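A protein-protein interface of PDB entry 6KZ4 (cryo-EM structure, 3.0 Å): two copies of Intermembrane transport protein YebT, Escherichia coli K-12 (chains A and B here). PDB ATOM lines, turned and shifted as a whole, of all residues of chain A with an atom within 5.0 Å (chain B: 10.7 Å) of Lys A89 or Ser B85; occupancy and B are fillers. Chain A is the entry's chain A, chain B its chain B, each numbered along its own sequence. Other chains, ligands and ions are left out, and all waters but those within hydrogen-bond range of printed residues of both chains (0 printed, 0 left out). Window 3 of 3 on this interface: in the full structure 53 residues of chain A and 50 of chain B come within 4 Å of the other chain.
Gln A17 touches Arg B86, but with the chains exchanged Arg A86 does not touch Gln B17 (19.3 Å).
Leu A88 touches Ser B85, but with the chains exchanged Ser A85 does not touch Leu B88 (11.8 Å).
Lys A89 touches Ser B85, but with the chains exchanged Ser A85 does not touch Lys B89 (14.4 Å).
Of the 7 pairs that touch across the chains among the printed residues, none has its exchanged pair printed and touching as well.
N of Gln A17 sits at hydrogen-bond distance from OG of Ser A20 (2.9 Å).
The backbone carbonyl oxygen (O) of Lys A89 lies within hydrogen-bond range of the side-chain hydroxyl (OG) of Ser A20 (2.6 Å).
NZ of Lys B26 lies within salt-bridge range of OE1 of Glu B65, at 3.1 Å.
Hydrophobic or aromatic side chains of chain B within 4 Å of the printed part of chain A: Leu B84.
Of the 13 printed residues of chain A, 5 touch a printed residue of chain B.
Hydrophobic or aromatic side chains of chain A within 4 Å of the printed part of chain B: Leu A88.
Among the printed residues, Asp or Glu carboxylates within 4 Å of a Lys or Arg side-chain nitrogen of the other chain: Asp A15 with Lys B26 (3.2 Å).
O of Ala A87 touches CB of Leu B84, at 3.0 Å.
Leu A88 touches Leu B84 (O to N, 3.7 Å).
The side-chain carboxylate of Asp A15 is in salt-bridge range of the side-chain amino group of Lys B26.
OD2 of Asp A15 sits close to OG of Ser B82, 3.4 Å away.
The side-chain amide nitrogen (NE2) of Gln A17 sits close to the guanidinium group (NE) of Arg B86 (3.0 Å).
The backbone carbonyl oxygen (O) of Leu A88 is in hydrogen-bond range of the side-chain hydroxyl (OG) of Ser B85, 3.0 Å away.
OG of Ser B85 is in hydrogen-bond range of NZ of Lys A89, 3.4 Å away.
Lys A89 touches just one residue of chain B: Ser B85 (3.4 Å).
Ser B85 touches just these residues of chain A: Leu A88 and Lys A89.
No residue of chain B comes within 4 Å of Val A16.
Gln A17 touches just one residue of chain B: Arg B86.
No residue of chain B comes within 4 Å of Ala A18.
No residue of chain B comes within 4 Å of Ser A85.
Of chain B, only Leu B84 and Ser B85 come within 4 Å of Leu A88.
Of the printed residues of chain B, Asp A15 touches Lys B26 and Ser B82.
Printed residues of chain A within 4 Å of Lys B26: Asp A15.
Of the printed residues of chain A, Ser B82 touches Asp A15.
Of the printed residues of chain A, Leu B84 touches Ala A87 and Leu A88.
The nearest printed residue of chain B that does not touch Lys A89 is Leu B84 (5.3 Å).
The nearest residue of chain A that does not touch Ser B85 is Gln A17 (4.2 Å).
The nearest printed residue of chain B that does not touch Asp A15 is Pro B83 (5.0 Å).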
ATOM      1  N   ASP A  15      21.604   4.529  24.047  1.00  0.00           N
ATOM      2  CA  ASP A  15      22.959   4.022  24.269  1.00  0.00           C
ATOM      3  C   ASP A  15      23.508   4.455  25.626  1.00  0.00           C
ATOM      4  O   ASP A  15      24.529   5.137  25.720  1.00  0.00           O
ATOM      5  CB  ASP A  15      23.897   4.462  23.145  1.00  0.00           C
ATOM      6  CG  ASP A  15      23.387   4.071  21.778  1.00  0.00           C
ATOM      7  OD1 ASP A  15      22.750   4.919  21.121  1.00  0.00           O
ATOM      8  OD2 ASP A  15      23.633   2.923  21.355  1.00  0.00           O
ATOM      9  N   VAL A  16      22.813   4.061  26.688  1.00  0.00           N
ATOM     10  CA  VAL A  16      23.262   4.317  28.048  1.00  0.00           C
ATOM     11  C   VAL A  16      23.110   3.039  28.857  1.00  0.00           C
ATOM     12  O   VAL A  16      22.199   2.239  28.628  1.00  0.00           O
ATOM     13  CB  VAL A  16      22.492   5.480  28.710  1.00  0.00           C
ATOM     14  CG1 VAL A  16      22.731   6.766  27.956  1.00  0.00           C
ATOM     15  CG2 VAL A  16      21.013   5.173  28.762  1.00  0.00           C
ATOM     16  N   GLN A  17      24.029   2.839  29.798  1.00  0.00           N
ATOM     17  CA  GLN A  17      23.981   1.674  30.670  1.00  0.00           C
ATOM     18  C   GLN A  17      24.166   2.086  32.120  1.00  0.00           C
ATOM     19  O   GLN A  17      24.224   3.278  32.434  1.00  0.00           O
ATOM     20  CB  GLN A  17      25.066   0.662  30.306  1.00  0.00           C
ATOM     21  CG  GLN A  17      25.405   0.568  28.841  1.00  0.00           C
ATOM     22  CD  GLN A  17      26.694  -0.185  28.612  1.00  0.00           C
ATOM     23  OE1 GLN A  17      27.576  -0.192  29.468  1.00  0.00           O
ATOM     24  NE2 GLN A  17      26.813  -0.822  27.458  1.00  0.00           N
ATOM     25  N   ALA A  18      24.274   1.104  33.005  1.00  0.00           N
ATOM     26  CA  ALA A  18      24.691   1.351  34.378  1.00  0.00           C
ATOM     27  C   ALA A  18      26.180   1.661  34.366  1.00  0.00           C
ATOM     28  O   ALA A  18      26.995   0.808  34.002  1.00  0.00           O
ATOM     29  CB  ALA A  18      24.381   0.145  35.257  1.00  0.00           C
ATOM     30  N   GLY A  19      26.539   2.881  34.749  1.00  0.00           N
ATOM     31  CA  GLY A  19      27.921   3.322  34.710  1.00  0.00           C
ATOM     32  C   GLY A  19      28.222   4.369  33.661  1.00  0.00           C
ATOM     33  O   GLY A  19      29.373   4.817  33.577  1.00  0.00           O
ATOM     34  N   SER A  20      27.253   4.773  32.845  1.00  0.00           N
ATOM     35  CA  SER A  20      27.485   5.839  31.883  1.00  0.00           C
ATOM     36  C   SER A  20      27.752   7.147  32.611  1.00  0.00           C
ATOM     37  O   SER A  20      27.065   7.491  33.574  1.00  0.00           O
ATOM     38  CB  SER A  20      26.281   5.990  30.960  1.00  0.00           C
ATOM     39  OG  SER A  20      26.081   4.817  30.195  1.00  0.00           O
ATOM     40  N   SER A  85      34.902   6.516  30.770  1.00  0.00           N
ATOM     41  CA  SER A  85      33.572   5.935  30.879  1.00  0.00           C
ATOM     42  C   SER A  85      32.670   6.365  29.735  1.00  0.00           C
ATOM     43  O   SER A  85      31.691   5.675  29.432  1.00  0.00           O
ATOM     44  CB  SER A  85      32.940   6.312  32.217  1.00  0.00           C
ATOM     45  OG  SER A  85      33.368   5.433  33.241  1.00  0.00           O
ATOM     46  N   ARG A  86      32.972   7.494  29.095  1.00  0.00           N
ATOM     47  CA  ARG A  86      32.210   7.893  27.917  1.00  0.00           C
ATOM     48  C   ARG A  86      32.495   6.965  26.750  1.00  0.00           C
ATOM     49  O   ARG A  86      31.578   6.394  26.155  1.00  0.00           O
ATOM     50  CB  ARG A  86      32.531   9.335  27.539  1.00  0.00           C
ATOM     51  CG  ARG A  86      31.813   9.810  26.295  1.00  0.00           C
ATOM     52  CD  ARG A  86      32.502  11.003  25.678  1.00  0.00           C
ATOM     53  NE  ARG A  86      31.997  11.272  24.338  1.00  0.00           N
ATOM     54  CZ  ARG A  86      31.412  12.407  23.978  1.00  0.00           C
ATOM     55  NH1 ARG A  86      30.982  12.568  22.736  1.00  0.00           N
ATOM     56  NH2 ARG A  86      31.259  13.382  24.860  1.00  0.00           N
ATOM     57  N   ALA A  87      33.761   6.787  26.425  1.00  0.00           N
ATOM     58  CA  ALA A  87      34.152   5.902  25.343  1.00  0.00           C
ATOM     59  C   ALA A  87      33.961   4.467  25.670  1.00  0.00           C
ATOM     60  O   ALA A  87      34.407   3.652  24.875  1.00  0.00           O
ATOM     61  CB  ALA A  87      35.612   6.150  24.966  1.00  0.00           C
ATOM     62  N   LEU A  88      33.346   4.098  26.774  1.00  0.00           N
ATOM     63  CA  LEU A  88      33.197   2.688  27.108  1.00  0.00           C
ATOM     64  C   LEU A  88      31.760   2.295  27.408  1.00  0.00           C
ATOM     65  O   LEU A  88      31.338   1.204  27.025  1.00  0.00           O
ATOM     66  CB  LEU A  88      34.092   2.349  28.301  1.00  0.00           C
ATOM     67  CG  LEU A  88      34.551   0.900  28.402  1.00  0.00           C
ATOM     68  CD1 LEU A  88      35.231   0.492  27.118  1.00  0.00           C
ATOM     69  CD2 LEU A  88      35.494   0.741  29.577  1.00  0.00           C
ATOM     70  N   LYS A  89      30.993   3.158  28.069  1.00  0.00           N
ATOM     71  CA  LYS A  89      29.608   2.853  28.387  1.00  0.00           C
ATOM     72  C   LYS A  89      28.619   3.924  27.957  1.00  0.00           C
ATOM     73  O   LYS A  89      27.431   3.788  28.262  1.00  0.00           O
ATOM     74  CB  LYS A  89      29.442   2.608  29.892  1.00  0.00           C
ATOM     75  CG  LYS A  89      30.245   1.440  30.414  1.00  0.00           C
ATOM     76  CD  LYS A  89      29.889   1.124  31.847  1.00  0.00           C
ATOM     77  CE  LYS A  89      30.812   0.064  32.410  1.00  0.00           C
ATOM     78  NZ  LYS A  89      30.940  -1.093  31.485  1.00  0.00           N
ATOM     79  N   GLY A  90      29.055   4.965  27.274  1.00  0.00           N
ATOM     80  CA  GLY A  90      28.181   6.041  26.861  1.00  0.00           C
ATOM     81  C   GLY A  90      28.316   7.238  27.782  1.00  0.00           C
ATOM     82  O   GLY A  90      29.147   7.274  28.690  1.00  0.00           O
ATOM     83  N   ALA A  91      27.466   8.230  27.537  1.00  0.00           N
ATOM     84  CA  ALA A  91      27.473   9.440  28.343  1.00  0.00           C
ATOM     85  C   ALA A  91      26.099  10.083  28.296  1.00  0.00           C
ATOM     86  O   ALA A  91      25.264   9.755  27.451  1.00  0.00           O
ATOM     87  CB  ALA A  91      28.539  10.428  27.867  1.00  0.00           C
ATOM     88  N   GLN B  17      29.023 -13.354  17.987  1.00  0.00           N
ATOM     89  CA  GLN B  17      29.649 -14.572  18.468  1.00  0.00           C
ATOM     90  C   GLN B  17      29.057 -14.914  19.823  1.00  0.00           C
ATOM     91  O   GLN B  17      28.227 -14.179  20.362  1.00  0.00           O
ATOM     92  CB  GLN B  17      31.164 -14.400  18.557  1.00  0.00           C
ATOM     93  CG  GLN B  17      31.580 -13.269  19.478  1.00  0.00           C
ATOM     94  CD  GLN B  17      33.001 -12.812  19.239  1.00  0.00           C
ATOM     95  OE1 GLN B  17      33.728 -13.400  18.439  1.00  0.00           O
ATOM     96  NE2 GLN B  17      33.405 -11.752  19.926  1.00  0.00           N
ATOM     97  N   GLY B  19      28.621 -14.826  23.502  1.00  0.00           N
ATOM     98  CA  GLY B  19      28.892 -13.763  24.447  1.00  0.00           C
ATOM     99  C   GLY B  19      28.309 -12.425  24.062  1.00  0.00           C
ATOM    100  O   GLY B  19      28.198 -11.548  24.926  1.00  0.00           O
ATOM    101  N   SER B  20      27.936 -12.239  22.800  1.00  0.00           N
ATOM    102  CA  SER B  20      27.298 -11.000  22.384  1.00  0.00           C
ATOM    103  C   SER B  20      25.971 -10.824  23.106  1.00  0.00           C
ATOM    104  O   SER B  20      25.281 -11.794  23.423  1.00  0.00           O
ATOM    105  CB  SER B  20      27.076 -11.000  20.876  1.00  0.00           C
ATOM    106  OG  SER B  20      28.232 -11.453  20.197  1.00  0.00           O
ATOM    107  N   VAL B  21      25.615  -9.582  23.364  1.00  0.00           N
ATOM    108  CA  VAL B  21      24.416  -9.271  24.130  1.00  0.00           C
ATOM    109  C   VAL B  21      23.232  -9.137  23.188  1.00  0.00           C
ATOM    110  O   VAL B  21      23.354  -8.610  22.081  1.00  0.00           O
ATOM    111  CB  VAL B  21      24.616  -7.990  24.958  1.00  0.00           C
ATOM    112  CG1 VAL B  21      25.475  -8.281  26.166  1.00  0.00           C
ATOM    113  CG2 VAL B  21      25.255  -6.916  24.114  1.00  0.00           C
ATOM    114  N   VAL B  22      22.080  -9.622  23.631  1.00  0.00           N
ATOM    115  CA  VAL B  22      20.820  -9.437  22.925  1.00  0.00           C
ATOM    116  C   VAL B  22      20.041  -8.384  23.692  1.00  0.00           C
ATOM    117  O   VAL B  22      19.522  -8.652  24.779  1.00  0.00           O
ATOM    118  CB  VAL B  22      20.029 -10.744  22.816  1.00  0.00           C
ATOM    119  CG1 VAL B  22      18.650 -10.471  22.267  1.00  0.00           C
ATOM    120  CG2 VAL B  22      20.760 -11.725  21.941  1.00  0.00           C
ATOM    121  N   LEU B  23      19.952  -7.184  23.134  1.00  0.00           N
ATOM    122  CA  LEU B  23      19.403  -6.039  23.840  1.00  0.00           C
ATOM    123  C   LEU B  23      18.052  -5.635  23.266  1.00  0.00           C
ATOM    124  O   LEU B  23      17.885  -5.540  22.048  1.00  0.00           O
ATOM    125  CB  LEU B  23      20.402  -4.878  23.804  1.00  0.00           C
ATOM    126  CG  LEU B  23      21.022  -4.500  22.463  1.00  0.00           C
ATOM    127  CD1 LEU B  23      20.202  -3.474  21.715  1.00  0.00           C
ATOM    128  CD2 LEU B  23      22.436  -4.007  22.671  1.00  0.00           C
ATOM    129  N   LYS B  26      17.253  -1.104  23.006  1.00  0.00           N
ATOM    130  CA  LYS B  26      18.619  -0.731  23.361  1.00  0.00           C
ATOM    131  C   LYS B  26      19.086  -1.357  24.668  1.00  0.00           C
ATOM    132  O   LYS B  26      20.196  -1.048  25.105  1.00  0.00           O
ATOM    133  CB  LYS B  26      18.810   0.787  23.429  1.00  0.00           C
ATOM    134  CG  LYS B  26      19.249   1.438  22.118  1.00  0.00           C
ATOM    135  CD  LYS B  26      20.217   0.577  21.331  1.00  0.00           C
ATOM    136  CE  LYS B  26      21.596   0.580  21.947  1.00  0.00           C
ATOM    137  NZ  LYS B  26      22.599  -0.048  21.045  1.00  0.00           N
ATOM    138  N   GLU B  28      19.802  -4.463  27.446  1.00  0.00           N
ATOM    139  CA  GLU B  28      20.267  -5.845  27.399  1.00  0.00           C
ATOM    140  C   GLU B  28      19.299  -6.772  28.123  1.00  0.00           C
ATOM    141  O   GLU B  28      19.018  -6.583  29.310  1.00  0.00           O
ATOM    142  CB  GLU B  28      21.657  -5.943  28.013  1.00  0.00           C
ATOM    143  CG  GLU B  28      22.135  -7.358  28.213  1.00  0.00           C
ATOM    144  CD  GLU B  28      23.448  -7.416  28.958  1.00  0.00           C
ATOM    145  OE1 GLU B  28      24.084  -6.353  29.117  1.00  0.00           O
ATOM    146  OE2 GLU B  28      23.841  -8.520  29.387  1.00  0.00           O
ATOM    147  N   GLU B  65      23.507  -5.378  15.179  1.00  0.00           N
ATOM    148  CA  GLU B  65      24.034  -4.028  15.306  1.00  0.00           C
ATOM    149  C   GLU B  65      25.531  -4.055  15.021  1.00  0.00           C
ATOM    150  O   GLU B  65      26.080  -5.046  14.534  1.00  0.00           O
ATOM    151  CB  GLU B  65      23.725  -3.458  16.685  1.00  0.00           C
ATOM    152  CG  GLU B  65      22.256  -3.199  16.928  1.00  0.00           C
ATOM    153  CD  GLU B  65      22.005  -2.530  18.257  1.00  0.00           C
ATOM    154  OE1 GLU B  65      22.975  -2.353  19.021  1.00  0.00           O
ATOM    155  OE2 GLU B  65      20.842  -2.177  18.539  1.00  0.00           O
ATOM    156  N   GLY B  66      26.209  -2.962  15.322  1.00  0.00           N
ATOM    157  CA  GLY B  66      27.643  -2.903  15.159  1.00  0.00           C
ATOM    158  C   GLY B  66      28.050  -1.948  14.050  1.00  0.00           C
ATOM    159  O   GLY B  66      27.243  -1.517  13.224  1.00  0.00           O
ATOM    160  N   GLN B  80      31.106   8.141  14.525  1.00  0.00           N
ATOM    161  CA  GLN B  80      30.647   7.859  15.876  1.00  0.00           C
ATOM    162  C   GLN B  80      30.820   6.377  16.174  1.00  0.00           C
ATOM    163  O   GLN B  80      30.624   5.530  15.300  1.00  0.00           O
ATOM    164  CB  GLN B  80      29.174   8.247  16.043  1.00  0.00           C
ATOM    165  CG  GLN B  80      28.604   8.059  17.434  1.00  0.00           C
ATOM    166  CD  GLN B  80      29.174   9.031  18.434  1.00  0.00           C
ATOM    167  OE1 GLN B  80      30.022   8.674  19.249  1.00  0.00           O
ATOM    168  NE2 GLN B  80      28.704  10.267  18.387  1.00  0.00           N
ATOM    169  N   ALA B  81      31.180   6.065  17.413  1.00  0.00           N
ATOM    170  CA  ALA B  81      31.404   4.687  17.842  1.00  0.00           C
ATOM    171  C   ALA B  81      30.663   4.429  19.147  1.00  0.00           C
ATOM    172  O   ALA B  81      31.225   3.918  20.114  1.00  0.00           O
ATOM    173  CB  ALA B  81      32.893   4.395  17.992  1.00  0.00           C
ATOM    174  N   SER B  82      29.375   4.787  19.167  1.00  0.00           N
ATOM    175  CA  SER B  82      28.587   4.928  20.399  1.00  0.00           C
ATOM    176  C   SER B  82      28.837   3.867  21.468  1.00  0.00           C
ATOM    177  O   SER B  82      29.035   4.243  22.632  1.00  0.00           O
ATOM    178  CB  SER B  82      27.099   4.985  20.023  1.00  0.00           C
ATOM    179  OG  SER B  82      26.289   5.113  21.178  1.00  0.00           O
ATOM    180  N   PRO B  83      28.826   2.570  21.182  1.00  0.00           N
ATOM    181  CA  PRO B  83      29.178   1.615  22.236  1.00  0.00           C
ATOM    182  C   PRO B  83      30.649   1.244  22.189  1.00  0.00           C
ATOM    183  O   PRO B  83      31.281   1.378  21.139  1.00  0.00           O
ATOM    184  CB  PRO B  83      28.283   0.412  21.920  1.00  0.00           C
ATOM    185  CG  PRO B  83      27.963   0.542  20.418  1.00  0.00           C
ATOM    186  CD  PRO B  83      28.478   1.873  19.932  1.00  0.00           C
ATOM    187  N   LEU B  84      31.223   0.795  23.303  1.00  0.00           N
ATOM    188  CA  LEU B  84      32.498   0.098  23.199  1.00  0.00           C
ATOM    189  C   LEU B  84      32.500  -1.132  24.095  1.00  0.00           C
ATOM    190  O   LEU B  84      33.208  -2.105  23.823  1.00  0.00           O
ATOM    191  CB  LEU B  84      33.663   1.018  23.544  1.00  0.00           C
ATOM    192  CG  LEU B  84      35.012   0.427  23.142  1.00  0.00           C
ATOM    193  CD1 LEU B  84      35.026   0.244  21.642  1.00  0.00           C
ATOM    194  CD2 LEU B  84      36.158   1.312  23.570  1.00  0.00           C
ATOM    195  N   SER B  85      31.709  -1.097  25.168  1.00  0.00           N
ATOM    196  CA  SER B  85      31.558  -2.287  25.994  1.00  0.00           C
ATOM    197  C   SER B  85      30.777  -3.366  25.263  1.00  0.00           C
ATOM    198  O   SER B  85      30.890  -4.548  25.599  1.00  0.00           O
ATOM    199  CB  SER B  85      30.877  -1.936  27.312  1.00  0.00           C
ATOM    200  OG  SER B  85      31.822  -1.465  28.254  1.00  0.00           O
ATOM    201  N   ARG B  86      29.984  -2.979  24.268  1.00  0.00           N
ATOM    202  CA  ARG B  86      29.295  -3.928  23.409  1.00  0.00           C
ATOM    203  C   ARG B  86      29.842  -3.953  21.992  1.00  0.00           C
ATOM    204  O   ARG B  86      29.614  -4.930  21.273  1.00  0.00           O
ATOM    205  CB  ARG B  86      27.799  -3.614  23.364  1.00  0.00           C
ATOM    206  CG  ARG B  86      27.137  -3.589  24.721  1.00  0.00           C
ATOM    207  CD  ARG B  86      25.755  -2.985  24.633  1.00  0.00           C
ATOM    208  NE  ARG B  86      25.138  -2.847  25.945  1.00  0.00           N
ATOM    209  CZ  ARG B  86      24.201  -1.954  26.235  1.00  0.00           C
ATOM    210  NH1 ARG B  86      23.776  -1.115  25.304  1.00  0.00           N
ATOM    211  NH2 ARG B  86      23.692  -1.899  27.456  1.00  0.00           N
ATOM    212  N   ALA B  87      30.551  -2.905  21.570  1.00  0.00           N
ATOM    213  CA  ALA B  87      31.126  -2.901  20.230  1.00  0.00           C
ATOM    214  C   ALA B  87      32.138  -4.024  20.059  1.00  0.00           C
ATOM    215  O   ALA B  87      32.145  -4.709  19.031  1.00  0.00           O
ATOM    216  CB  ALA B  87      31.772  -1.550  19.936  1.00  0.00           C
ATOM    217  N   LEU B  88      32.997  -4.232  21.051  1.00  0.00           N
ATOM    218  CA  LEU B  88      33.944  -5.335  21.012  1.00  0.00           C
ATOM    219  C   LEU B  88      33.336  -6.631  21.522  1.00  0.00           C
ATOM    220  O   LEU B  88      33.999  -7.672  21.491  1.00  0.00           O
ATOM    221  CB  LEU B  88      35.205  -4.989  21.811  1.00  0.00           C
ATOM    222  CG  LEU B  88      35.100  -4.784  23.321  1.00  0.00           C
ATOM    223  CD1 LEU B  88      35.436  -6.063  24.068  1.00  0.00           C
ATOM    224  CD2 LEU B  88      36.029  -3.668  23.751  1.00  0.00           C
ATOM    225  N   LYS B  89      32.090  -6.589  21.984  1.00  0.00           N
ATOM    226  CA  LYS B  89      31.376  -7.775  22.415  1.00  0.00           C
ATOM    227  C   LYS B  89      30.368  -8.274  21.397  1.00  0.00           C
ATOM    228  O   LYS B  89      29.997  -9.451  21.453  1.00  0.00           O
ATOM    229  CB  LYS B  89      30.645  -7.506  23.740  1.00  0.00           C
ATOM    230  CG  LYS B  89      30.476  -8.724  24.619  1.00  0.00           C
ATOM    231  CD  LYS B  89      31.816  -9.358  24.938  1.00  0.00           C
ATOM    232  CE  LYS B  89      31.643 -10.625  25.759  1.00  0.00           C
ATOM    233  NZ  LYS B  89      32.908 -11.402  25.857  1.00  0.00           N
ATOM    234  N   GLY B  90      29.926  -7.431  20.469  1.00  0.00           N
ATOM    235  CA  GLY B  90      28.885  -7.806  19.536  1.00  0.00           C
ATOM    236  C   GLY B  90      27.516  -7.675  20.164  1.00  0.00           C
ATOM    237  O   GLY B  90      27.362  -7.889  21.368  1.00  0.00           O
ATOM    238  N   ALA B  91      26.512  -7.319  19.369  1.00  0.00           N
ATOM    239  CA  ALA B  91      25.163  -7.134  19.885  1.00  0.00           C
ATOM    240  C   ALA B  91      24.174  -7.249  18.743  1.00  0.00           C
ATOM    241  O   ALA B  91      24.310  -6.554  17.734  1.00  0.00           O
ATOM    242  CB  ALA B  91      25.017  -5.777  20.576  1.00  0.00           C
